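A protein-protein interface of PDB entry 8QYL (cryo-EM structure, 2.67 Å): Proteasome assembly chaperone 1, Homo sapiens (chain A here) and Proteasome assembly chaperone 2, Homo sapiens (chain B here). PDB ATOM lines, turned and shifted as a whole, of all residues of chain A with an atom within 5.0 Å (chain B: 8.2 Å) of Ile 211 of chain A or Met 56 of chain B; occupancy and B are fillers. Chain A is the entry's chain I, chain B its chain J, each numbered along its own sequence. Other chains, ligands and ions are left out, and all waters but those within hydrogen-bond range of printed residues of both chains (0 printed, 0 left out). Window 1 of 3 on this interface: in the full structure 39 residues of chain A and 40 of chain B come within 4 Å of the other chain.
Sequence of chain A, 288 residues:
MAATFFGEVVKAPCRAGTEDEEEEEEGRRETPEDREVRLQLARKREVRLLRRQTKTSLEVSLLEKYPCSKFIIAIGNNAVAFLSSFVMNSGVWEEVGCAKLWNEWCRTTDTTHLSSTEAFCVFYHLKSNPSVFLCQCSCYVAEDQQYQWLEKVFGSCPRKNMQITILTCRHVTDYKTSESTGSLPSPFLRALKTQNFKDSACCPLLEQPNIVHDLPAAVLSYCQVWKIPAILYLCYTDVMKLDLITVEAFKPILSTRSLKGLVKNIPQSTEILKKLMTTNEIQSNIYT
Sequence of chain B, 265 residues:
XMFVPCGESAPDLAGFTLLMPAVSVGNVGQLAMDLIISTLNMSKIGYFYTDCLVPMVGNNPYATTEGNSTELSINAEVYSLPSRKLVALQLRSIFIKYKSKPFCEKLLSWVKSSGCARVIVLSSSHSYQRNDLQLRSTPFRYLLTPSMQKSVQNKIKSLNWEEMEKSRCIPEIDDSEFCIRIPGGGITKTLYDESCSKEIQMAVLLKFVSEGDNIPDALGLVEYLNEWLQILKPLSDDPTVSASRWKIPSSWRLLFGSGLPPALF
O of Ala 217 of chain A is in hydrogen-bond range of OG of Ser 221 of chain A, 2.6 Å away.
Of the printed residues of chain B, Gln 208 of chain A touches Asn 59. Asn 210 of chain A touches none of the printed residues of chain B. Ile 211 of chain A touches just these residues of chain B: Met 56 and Val 57. Of the printed residues of chain B, Ser 221 of chain A touches Met 56 (3.8 Å). Printed residues of chain A within 4 Å of Pro 55 of chain B: His 213 and Ala 217. Of chain A, only Ile 211 (3.8 Å), Val 212 (3.3 Å), Ala 217 (3.9 Å) and Ser 221 (3.8 Å) come within 4 Å of Met 56 of chain B. The nearest residue of chain A that does not touch Met 56 of chain B is His 213 of chain A (4.3 Å).
Printed residues of chain B that touch a printed residue of chain A: Pro 55, Met 56, Val 57 and Asn 59. Hydrophobic or aromatic side chains of chain B within 4 Å of the printed part of chain A: Met 56 and Val 57. Along chain B the printed residues that touch a printed residue of chain A span positions 55 to 59. Of the 9 printed residues of chain A, 7 touch a printed residue of chain B. Printed residues of chain A that touch a printed residue of chain B: Leu 206, Gln 208, Ile 211, Val 212, His 213, Ala 217 and Ser 221. Hydrophobic or aromatic side chains of chain A that line the printed part of chain B: Ile 211, Val 212, His 213 and Ala 217. Among the printed residues, no Asp or Glu carboxylate lies within 4 Å of a Lys or Arg side-chain nitrogen of the other chain.
Among the printed residues, merely in contact across the chains: Val 212 of chain A with Met 56 of chain B (3.3 Å), Gln 208 of chain A with Asn 59 of chain B (3.4 Å), His 213 of chain A with Pro 55 of chain B (3.5 Å), Ile 211 of chain A with Val 57 of chain B (3.5 Å), Ile 211 of chain A with Met 56 of chain B (3.8 Å), Ser 221 of chain A with Met 56 of chain B (3.8 Å), Ala 217 of chain A with Val 57 of chain B (3.8 Å), Ala 217 of chain A with Pro 55 of chain B (3.9 Å) and Ala 217 of chain A with Met 56 of chain B (3.9 Å).
ND2 of Asn 59 of chain B sits at hydrogen-bond distance from O of Leu 206 of chain A, 3.2 Å away. The backbone NH of Val 57 of chain B sits at hydrogen-bond distance from the backbone carbonyl oxygen of Val 212 of chain A, at 2.9 Å.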
ATOM      1  N   LEU A 206      13.812 -11.999  -3.894  1.00  0.00           N
ATOM      2  CA  LEU A 206      13.701 -13.136  -2.991  1.00  0.00           C
ATOM      3  C   LEU A 206      14.668 -12.989  -1.824  1.00  0.00           C
ATOM      4  O   LEU A 206      15.832 -12.623  -2.009  1.00  0.00           O
ATOM      5  CB  LEU A 206      13.971 -14.433  -3.753  1.00  0.00           C
ATOM      6  CG  LEU A 206      13.765 -15.756  -3.017  1.00  0.00           C
ATOM      7  CD1 LEU A 206      12.353 -15.862  -2.487  1.00  0.00           C
ATOM      8  CD2 LEU A 206      14.080 -16.924  -3.930  1.00  0.00           C
ATOM      9  N   GLN A 208      17.059 -13.974   1.522  1.00  0.00           N
ATOM     10  CA  GLN A 208      18.346 -14.658   1.388  1.00  0.00           C
ATOM     11  C   GLN A 208      18.235 -16.168   1.552  1.00  0.00           C
ATOM     12  O   GLN A 208      18.503 -16.894   0.578  1.00  0.00           O
ATOM     13  CB  GLN A 208      19.372 -14.037   2.336  1.00  0.00           C
ATOM     14  CG  GLN A 208      19.766 -12.626   1.942  1.00  0.00           C
ATOM     15  CD  GLN A 208      20.555 -12.579   0.655  1.00  0.00           C
ATOM     16  OE1 GLN A 208      20.973 -13.608   0.132  1.00  0.00           O
ATOM     17  NE2 GLN A 208      20.763 -11.379   0.134  1.00  0.00           N
ATOM     18  N   PRO A 209      17.825 -16.711   2.704  1.00  0.00           N
ATOM     19  CA  PRO A 209      17.946 -18.169   2.896  1.00  0.00           C
ATOM     20  C   PRO A 209      17.196 -18.992   1.863  1.00  0.00           C
ATOM     21  O   PRO A 209      17.468 -20.192   1.736  1.00  0.00           O
ATOM     22  CB  PRO A 209      17.378 -18.390   4.305  1.00  0.00           C
ATOM     23  CG  PRO A 209      17.397 -17.058   4.947  1.00  0.00           C
ATOM     24  CD  PRO A 209      17.166 -16.075   3.856  1.00  0.00           C
ATOM     25  N   ASN A 210      16.276 -18.390   1.114  1.00  0.00           N
ATOM     26  CA  ASN A 210      15.505 -19.107   0.110  1.00  0.00           C
ATOM     27  C   ASN A 210      16.296 -19.258  -1.183  1.00  0.00           C
ATOM     28  O   ASN A 210      16.997 -18.339  -1.611  1.00  0.00           O
ATOM     29  CB  ASN A 210      14.195 -18.375  -0.167  1.00  0.00           C
ATOM     30  CG  ASN A 210      13.342 -18.224   1.070  1.00  0.00           C
ATOM     31  OD1 ASN A 210      12.597 -19.129   1.434  1.00  0.00           O
ATOM     32  ND2 ASN A 210      13.442 -17.075   1.721  1.00  0.00           N
ATOM     33  N   ILE A 211      16.169 -20.429  -1.809  1.00  0.00           N
ATOM     34  CA  ILE A 211      16.834 -20.739  -3.068  1.00  0.00           C
ATOM     35  C   ILE A 211      15.830 -21.392  -4.008  1.00  0.00           C
ATOM     36  O   ILE A 211      14.763 -21.850  -3.599  1.00  0.00           O
ATOM     37  CB  ILE A 211      18.060 -21.659  -2.881  1.00  0.00           C
ATOM     38  CG1 ILE A 211      17.638 -22.990  -2.259  1.00  0.00           C
ATOM     39  CG2 ILE A 211      19.124 -20.980  -2.040  1.00  0.00           C
ATOM     40  CD1 ILE A 211      18.632 -24.097  -2.463  1.00  0.00           C
ATOM     41  N   VAL A 212      16.189 -21.426  -5.290  1.00  0.00           N
ATOM     42  CA  VAL A 212      15.369 -22.029  -6.333  1.00  0.00           C
ATOM     43  C   VAL A 212      16.205 -23.059  -7.075  1.00  0.00           C
ATOM     44  O   VAL A 212      17.386 -22.825  -7.354  1.00  0.00           O
ATOM     45  CB  VAL A 212      14.823 -20.972  -7.318  1.00  0.00           C
ATOM     46  CG1 VAL A 212      13.724 -21.563  -8.180  1.00  0.00           C
ATOM     47  CG2 VAL A 212      14.316 -19.758  -6.570  1.00  0.00           C
ATOM     48  N   HIS A 213      15.600 -24.203  -7.390  1.00  0.00           N
ATOM     49  CA  HIS A 213      16.290 -25.216  -8.179  1.00  0.00           C
ATOM     50  C   HIS A 213      15.437 -25.672  -9.358  1.00  0.00           C
ATOM     51  O   HIS A 213      14.407 -25.059  -9.654  1.00  0.00           O
ATOM     52  CB  HIS A 213      16.693 -26.406  -7.302  1.00  0.00           C
ATOM     53  CG  HIS A 213      15.542 -27.132  -6.681  1.00  0.00           C
ATOM     54  ND1 HIS A 213      14.700 -26.548  -5.760  1.00  0.00           N
ATOM     55  CD2 HIS A 213      15.107 -28.405  -6.833  1.00  0.00           C
ATOM     56  CE1 HIS A 213      13.789 -27.426  -5.381  1.00  0.00           C
ATOM     57  NE2 HIS A 213      14.013 -28.560  -6.017  1.00  0.00           N
ATOM     58  N   ALA A 217      16.029 -22.460 -12.483  1.00  0.00           N
ATOM     59  CA  ALA A 217      17.376 -22.202 -11.994  1.00  0.00           C
ATOM     60  C   ALA A 217      18.412 -22.492 -13.068  1.00  0.00           C
ATOM     61  O   ALA A 217      19.404 -21.768 -13.193  1.00  0.00           O
ATOM     62  CB  ALA A 217      17.649 -23.035 -10.746  1.00  0.00           C
ATOM     63  N   SER A 221      20.872 -19.639 -14.452  1.00  0.00           N
ATOM     64  CA  SER A 221      22.312 -19.843 -14.333  1.00  0.00           C
ATOM     65  C   SER A 221      22.997 -19.755 -15.688  1.00  0.00           C
ATOM     66  O   SER A 221      24.080 -19.168 -15.803  1.00  0.00           O
ATOM     67  CB  SER A 221      22.593 -21.193 -13.676  1.00  0.00           C
ATOM     68  OG  SER A 221      21.860 -21.332 -12.474  1.00  0.00           O
ATOM     69  N   LEU B  53      26.382 -31.035 -11.625  1.00  0.00           N
ATOM     70  CA  LEU B  53      25.651 -30.759 -10.397  1.00  0.00           C
ATOM     71  C   LEU B  53      24.249 -30.260 -10.713  1.00  0.00           C
ATOM     72  O   LEU B  53      24.024 -29.580 -11.717  1.00  0.00           O
ATOM     73  CB  LEU B  53      26.372 -29.725  -9.525  1.00  0.00           C
ATOM     74  CG  LEU B  53      27.578 -30.159  -8.688  1.00  0.00           C
ATOM     75  CD1 LEU B  53      28.815 -30.329  -9.549  1.00  0.00           C
ATOM     76  CD2 LEU B  53      27.838 -29.180  -7.561  1.00  0.00           C
ATOM     77  N   VAL B  54      23.308 -30.612  -9.841  1.00  0.00           N
ATOM     78  CA  VAL B  54      21.932 -30.122  -9.974  1.00  0.00           C
ATOM     79  C   VAL B  54      21.938 -28.600  -9.900  1.00  0.00           C
ATOM     80  O   VAL B  54      22.529 -28.029  -8.963  1.00  0.00           O
ATOM     81  CB  VAL B  54      21.041 -30.722  -8.874  1.00  0.00           C
ATOM     82  CG1 VAL B  54      19.614 -30.230  -9.016  1.00  0.00           C
ATOM     83  CG2 VAL B  54      21.093 -32.235  -8.919  1.00  0.00           C
ATOM     84  N   PRO B  55      21.317 -27.894 -10.843  1.00  0.00           N
ATOM     85  CA  PRO B  55      21.404 -26.429 -10.834  1.00  0.00           C
ATOM     86  C   PRO B  55      20.555 -25.808  -9.736  1.00  0.00           C
ATOM     87  O   PRO B  55      19.440 -26.253  -9.456  1.00  0.00           O
ATOM     88  CB  PRO B  55      20.896 -26.036 -12.225  1.00  0.00           C
ATOM     89  CG  PRO B  55      20.055 -27.173 -12.661  1.00  0.00           C
ATOM     90  CD  PRO B  55      20.613 -28.407 -12.029  1.00  0.00           C
ATOM     91  N   MET B  56      21.101 -24.763  -9.115  1.00  0.00           N
ATOM     92  CA  MET B  56      20.393 -23.982  -8.111  1.00  0.00           C
ATOM     93  C   MET B  56      20.850 -22.538  -8.221  1.00  0.00           C
ATOM     94  O   MET B  56      21.897 -22.244  -8.801  1.00  0.00           O
ATOM     95  CB  MET B  56      20.627 -24.520  -6.693  1.00  0.00           C
ATOM     96  CG  MET B  56      22.084 -24.721  -6.323  1.00  0.00           C
ATOM     97  SD  MET B  56      22.844 -23.259  -5.595  1.00  0.00           S
ATOM     98  CE  MET B  56      21.783 -22.984  -4.185  1.00  0.00           C
ATOM     99  N   VAL B  57      20.053 -21.629  -7.659  1.00  0.00           N
ATOM    100  CA  VAL B  57      20.326 -20.202  -7.772  1.00  0.00           C
ATOM    101  C   VAL B  57      19.817 -19.504  -6.517  1.00  0.00           C
ATOM    102  O   VAL B  57      18.899 -19.981  -5.848  1.00  0.00           O
ATOM    103  CB  VAL B  57      19.687 -19.618  -9.058  1.00  0.00           C
ATOM    104  CG1 VAL B  57      18.169 -19.662  -8.980  1.00  0.00           C
ATOM    105  CG2 VAL B  57      20.194 -18.219  -9.341  1.00  0.00           C
ATOM    106  N   GLY B  58      20.435 -18.375  -6.193  1.00  0.00           N
ATOM    107  CA  GLY B  58      20.048 -17.603  -5.026  1.00  0.00           C
ATOM    108  C   GLY B  58      20.831 -16.310  -4.981  1.00  0.00           C
ATOM    109  O   GLY B  58      21.697 -16.050  -5.821  1.00  0.00           O
ATOM    110  N   ASN B  59      20.516 -15.493  -3.979  1.00  0.00           N
ATOM    111  CA  ASN B  59      21.179 -14.210  -3.810  1.00  0.00           C
ATOM    112  C   ASN B  59      22.465 -14.380  -3.003  1.00  0.00           C
ATOM    113  O   ASN B  59      22.850 -15.488  -2.628  1.00  0.00           O
ATOM    114  CB  ASN B  59      20.238 -13.205  -3.153  1.00  0.00           C
ATOM    115  CG  ASN B  59      19.576 -12.283  -4.156  1.00  0.00           C
ATOM    116  OD1 ASN B  59      20.166 -11.928  -5.172  1.00  0.00           O
ATOM    117  ND2 ASN B  59      18.343 -11.888  -3.874  1.00  0.00           N
ATOM    118  N   PRO B  61      25.220 -14.975  -0.510  1.00  0.00           N
ATOM    119  CA  PRO B  61      25.235 -15.600   0.817  1.00  0.00           C
ATOM    120  C   PRO B  61      26.139 -14.921   1.833  1.00  0.00           C
ATOM    121  O   PRO B  61      26.161 -15.351   2.992  1.00  0.00           O
ATOM    122  CB  PRO B  61      25.733 -17.026   0.520  1.00  0.00           C
ATOM    123  CG  PRO B  61      25.677 -17.178  -0.962  1.00  0.00           C
ATOM    124  CD  PRO B  61      25.886 -15.817  -1.511  1.00  0.00           C
ATOM    125  N   LEU B  72      23.508 -12.236  -7.715  1.00  0.00           N
ATOM    126  CA  LEU B  72      23.095 -13.608  -7.971  1.00  0.00           C
ATOM    127  C   LEU B  72      24.259 -14.574  -7.785  1.00  0.00           C
ATOM    128  O   LEU B  72      25.416 -14.251  -8.061  1.00  0.00           O
ATOM    129  CB  LEU B  72      22.533 -13.731  -9.385  1.00  0.00           C
ATOM    130  CG  LEU B  72      21.502 -14.833  -9.612  1.00  0.00           C
ATOM    131  CD1 LEU B  72      20.190 -14.478  -8.942  1.00  0.00           C
ATOM    132  CD2 LEU B  72      21.305 -15.069 -11.097  1.00  0.00           C
ATOM    133  N   SER B  73      23.936 -15.779  -7.316  1.00  0.00           N
ATOM    134  CA  SER B  73      24.919 -16.825  -7.083  1.00  0.00           C
ATOM    135  C   SER B  73      24.451 -18.128  -7.714  1.00  0.00           C
ATOM    136  O   SER B  73      23.252 -18.400  -7.796  1.00  0.00           O
ATOM    137  CB  SER B  73      25.166 -17.039  -5.586  1.00  0.00           C
ATOM    138  OG  SER B  73      25.870 -15.948  -5.021  1.00  0.00           O
ATOM    139  N   ILE B  74      25.414 -18.939  -8.152  1.00  0.00           N
ATOM    140  CA  ILE B  74      25.120 -20.231  -8.765  1.00  0.00           C
ATOM    141  C   ILE B  74      25.793 -21.332  -7.953  1.00  0.00           C
ATOM    142  O   ILE B  74      26.425 -21.059  -6.928  1.00  0.00           O
ATOM    143  CB  ILE B  74      25.555 -20.269 -10.243  1.00  0.00           C
ATOM    144  CG1 ILE B  74      27.074 -20.365 -10.364  1.00  0.00           C
ATOM    145  CG2 ILE B  74      25.042 -19.046 -10.982  1.00  0.00           C
ATOM    146  CD1 ILE B  74      27.532 -21.041 -11.632  1.00  0.00           C
ATOM    147  N   ASN B  75      25.659 -22.584  -8.399  1.00  0.00           N
ATOM    148  CA  ASN B  75      26.037 -23.716  -7.559  1.00  0.00           C
ATOM    149  C   ASN B  75      27.545 -23.915  -7.445  1.00  0.00           C
ATOM    150  O   ASN B  75      27.985 -24.656  -6.561  1.00  0.00           O
ATOM    151  CB  ASN B  75      25.388 -25.000  -8.078  1.00  0.00           C
ATOM    152  CG  ASN B  75      25.640 -25.227  -9.549  1.00  0.00           C
ATOM    153  OD1 ASN B  75      26.381 -24.483 -10.188  1.00  0.00           O
ATOM    154  ND2 ASN B  75      25.023 -26.264 -10.100  1.00  0.00           N
ATOM    155  N   ALA B  76      28.346 -23.289  -8.305  1.00  0.00           N
ATOM    156  CA  ALA B  76      29.799 -23.427  -8.239  1.00  0.00           C
ATOM    157  C   ALA B  76      30.442 -22.087  -8.549  1.00  0.00           C
ATOM    158  O   ALA B  76      30.206 -21.521  -9.619  1.00  0.00           O
ATOM    159  CB  ALA B  76      30.300 -24.500  -9.207  1.00  0.00           C
ATOM    160  N   GLU B  77      31.260 -21.589  -7.625  1.00  0.00           N
ATOM    161  CA  GLU B  77      31.894 -20.288  -7.773  1.00  0.00           C
ATOM    162  C   GLU B  77      33.316 -20.348  -7.242  1.00  0.00           C
ATOM    163  O   GLU B  77      33.654 -21.186  -6.405  1.00  0.00           O
ATOM    164  CB  GLU B  77      31.106 -19.195  -7.049  1.00  0.00           C
ATOM    165  CG  GLU B  77      30.043 -18.554  -7.908  1.00  0.00           C
ATOM    166  CD  GLU B  77      28.880 -18.041  -7.098  1.00  0.00           C
ATOM    167  OE1 GLU B  77      28.851 -18.285  -5.874  1.00  0.00           O
ATOM    168  OE2 GLU B  77      27.994 -17.390  -7.685  1.00  0.00           O
ATOM    169  N   LEU B  91      31.018 -25.481  -3.670  1.00  0.00           N
ATOM    170  CA  LEU B  91      29.927 -26.189  -4.329  1.00  0.00           C
ATOM    171  C   LEU B  91      28.712 -26.181  -3.414  1.00  0.00           C
ATOM    172  O   LEU B  91      28.826 -26.501  -2.228  1.00  0.00           O
ATOM    173  CB  LEU B  91      30.324 -27.626  -4.664  1.00  0.00           C
ATOM    174  CG  LEU B  91      31.627 -27.830  -5.431  1.00  0.00           C
ATOM    175  CD1 LEU B  91      31.944 -29.306  -5.546  1.00  0.00           C
ATOM    176  CD2 LEU B  91      31.535 -27.199  -6.802  1.00  0.00           C
ATOM    177  N   ARG B  92      27.551 -25.829  -3.964  1.00  0.00           N
ATOM    178  CA  ARG B  92      26.352 -25.617  -3.160  1.00  0.00           C
ATOM    179  C   ARG B  92      25.232 -26.605  -3.459  1.00  0.00           C
ATOM    180  O   ARG B  92      24.111 -26.407  -2.983  1.00  0.00           O
ATOM    181  CB  ARG B  92      25.837 -24.189  -3.349  1.00  0.00           C
ATOM    182  CG  ARG B  92      26.786 -23.128  -2.847  1.00  0.00           C
ATOM    183  CD  ARG B  92      26.081 -21.807  -2.636  1.00  0.00           C
ATOM    184  NE  ARG B  92      27.010 -20.763  -2.228  1.00  0.00           N
ATOM    185  CZ  ARG B  92      27.805 -20.102  -3.057  1.00  0.00           C
ATOM    186  NH1 ARG B  92      27.801 -20.343  -4.357  1.00  0.00           N
ATOM    187  NH2 ARG B  92      28.624 -19.175  -2.572  1.00  0.00           N
ATOM    188  N   SER B  93      25.495 -27.661  -4.223  1.00  0.00           N
ATOM    189  CA  SER B  93      24.460 -28.627  -4.567  1.00  0.00           C
ATOM    190  C   SER B  93      25.077 -30.020  -4.558  1.00  0.00           C
ATOM    191  O   SER B  93      26.184 -30.230  -4.056  1.00  0.00           O
ATOM    192  CB  SER B  93      23.816 -28.281  -5.916  1.00  0.00           C
ATOM    193  OG  SER B  93      24.776 -28.291  -6.953  1.00  0.00           O
ATOM    194  N   ILE B  94      24.349 -30.983  -5.117  1.00  0.00           N
ATOM    195  CA  ILE B  94      24.767 -32.380  -5.108  1.00  0.00           C
ATOM    196  C   ILE B  94      24.975 -32.873  -6.534  1.00  0.00           C
ATOM    197  O   ILE B  94      24.758 -32.132  -7.497  1.00  0.00           O
ATOM    198  CB  ILE B  94      23.741 -33.243  -4.354  1.00  0.00           C
ATOM    199  CG1 ILE B  94      22.366 -33.097  -4.993  1.00  0.00           C
ATOM    200  CG2 ILE B  94      23.683 -32.857  -2.887  1.00  0.00           C
ATOM    201  CD1 ILE B  94      21.357 -34.018  -4.416  1.00  0.00           C
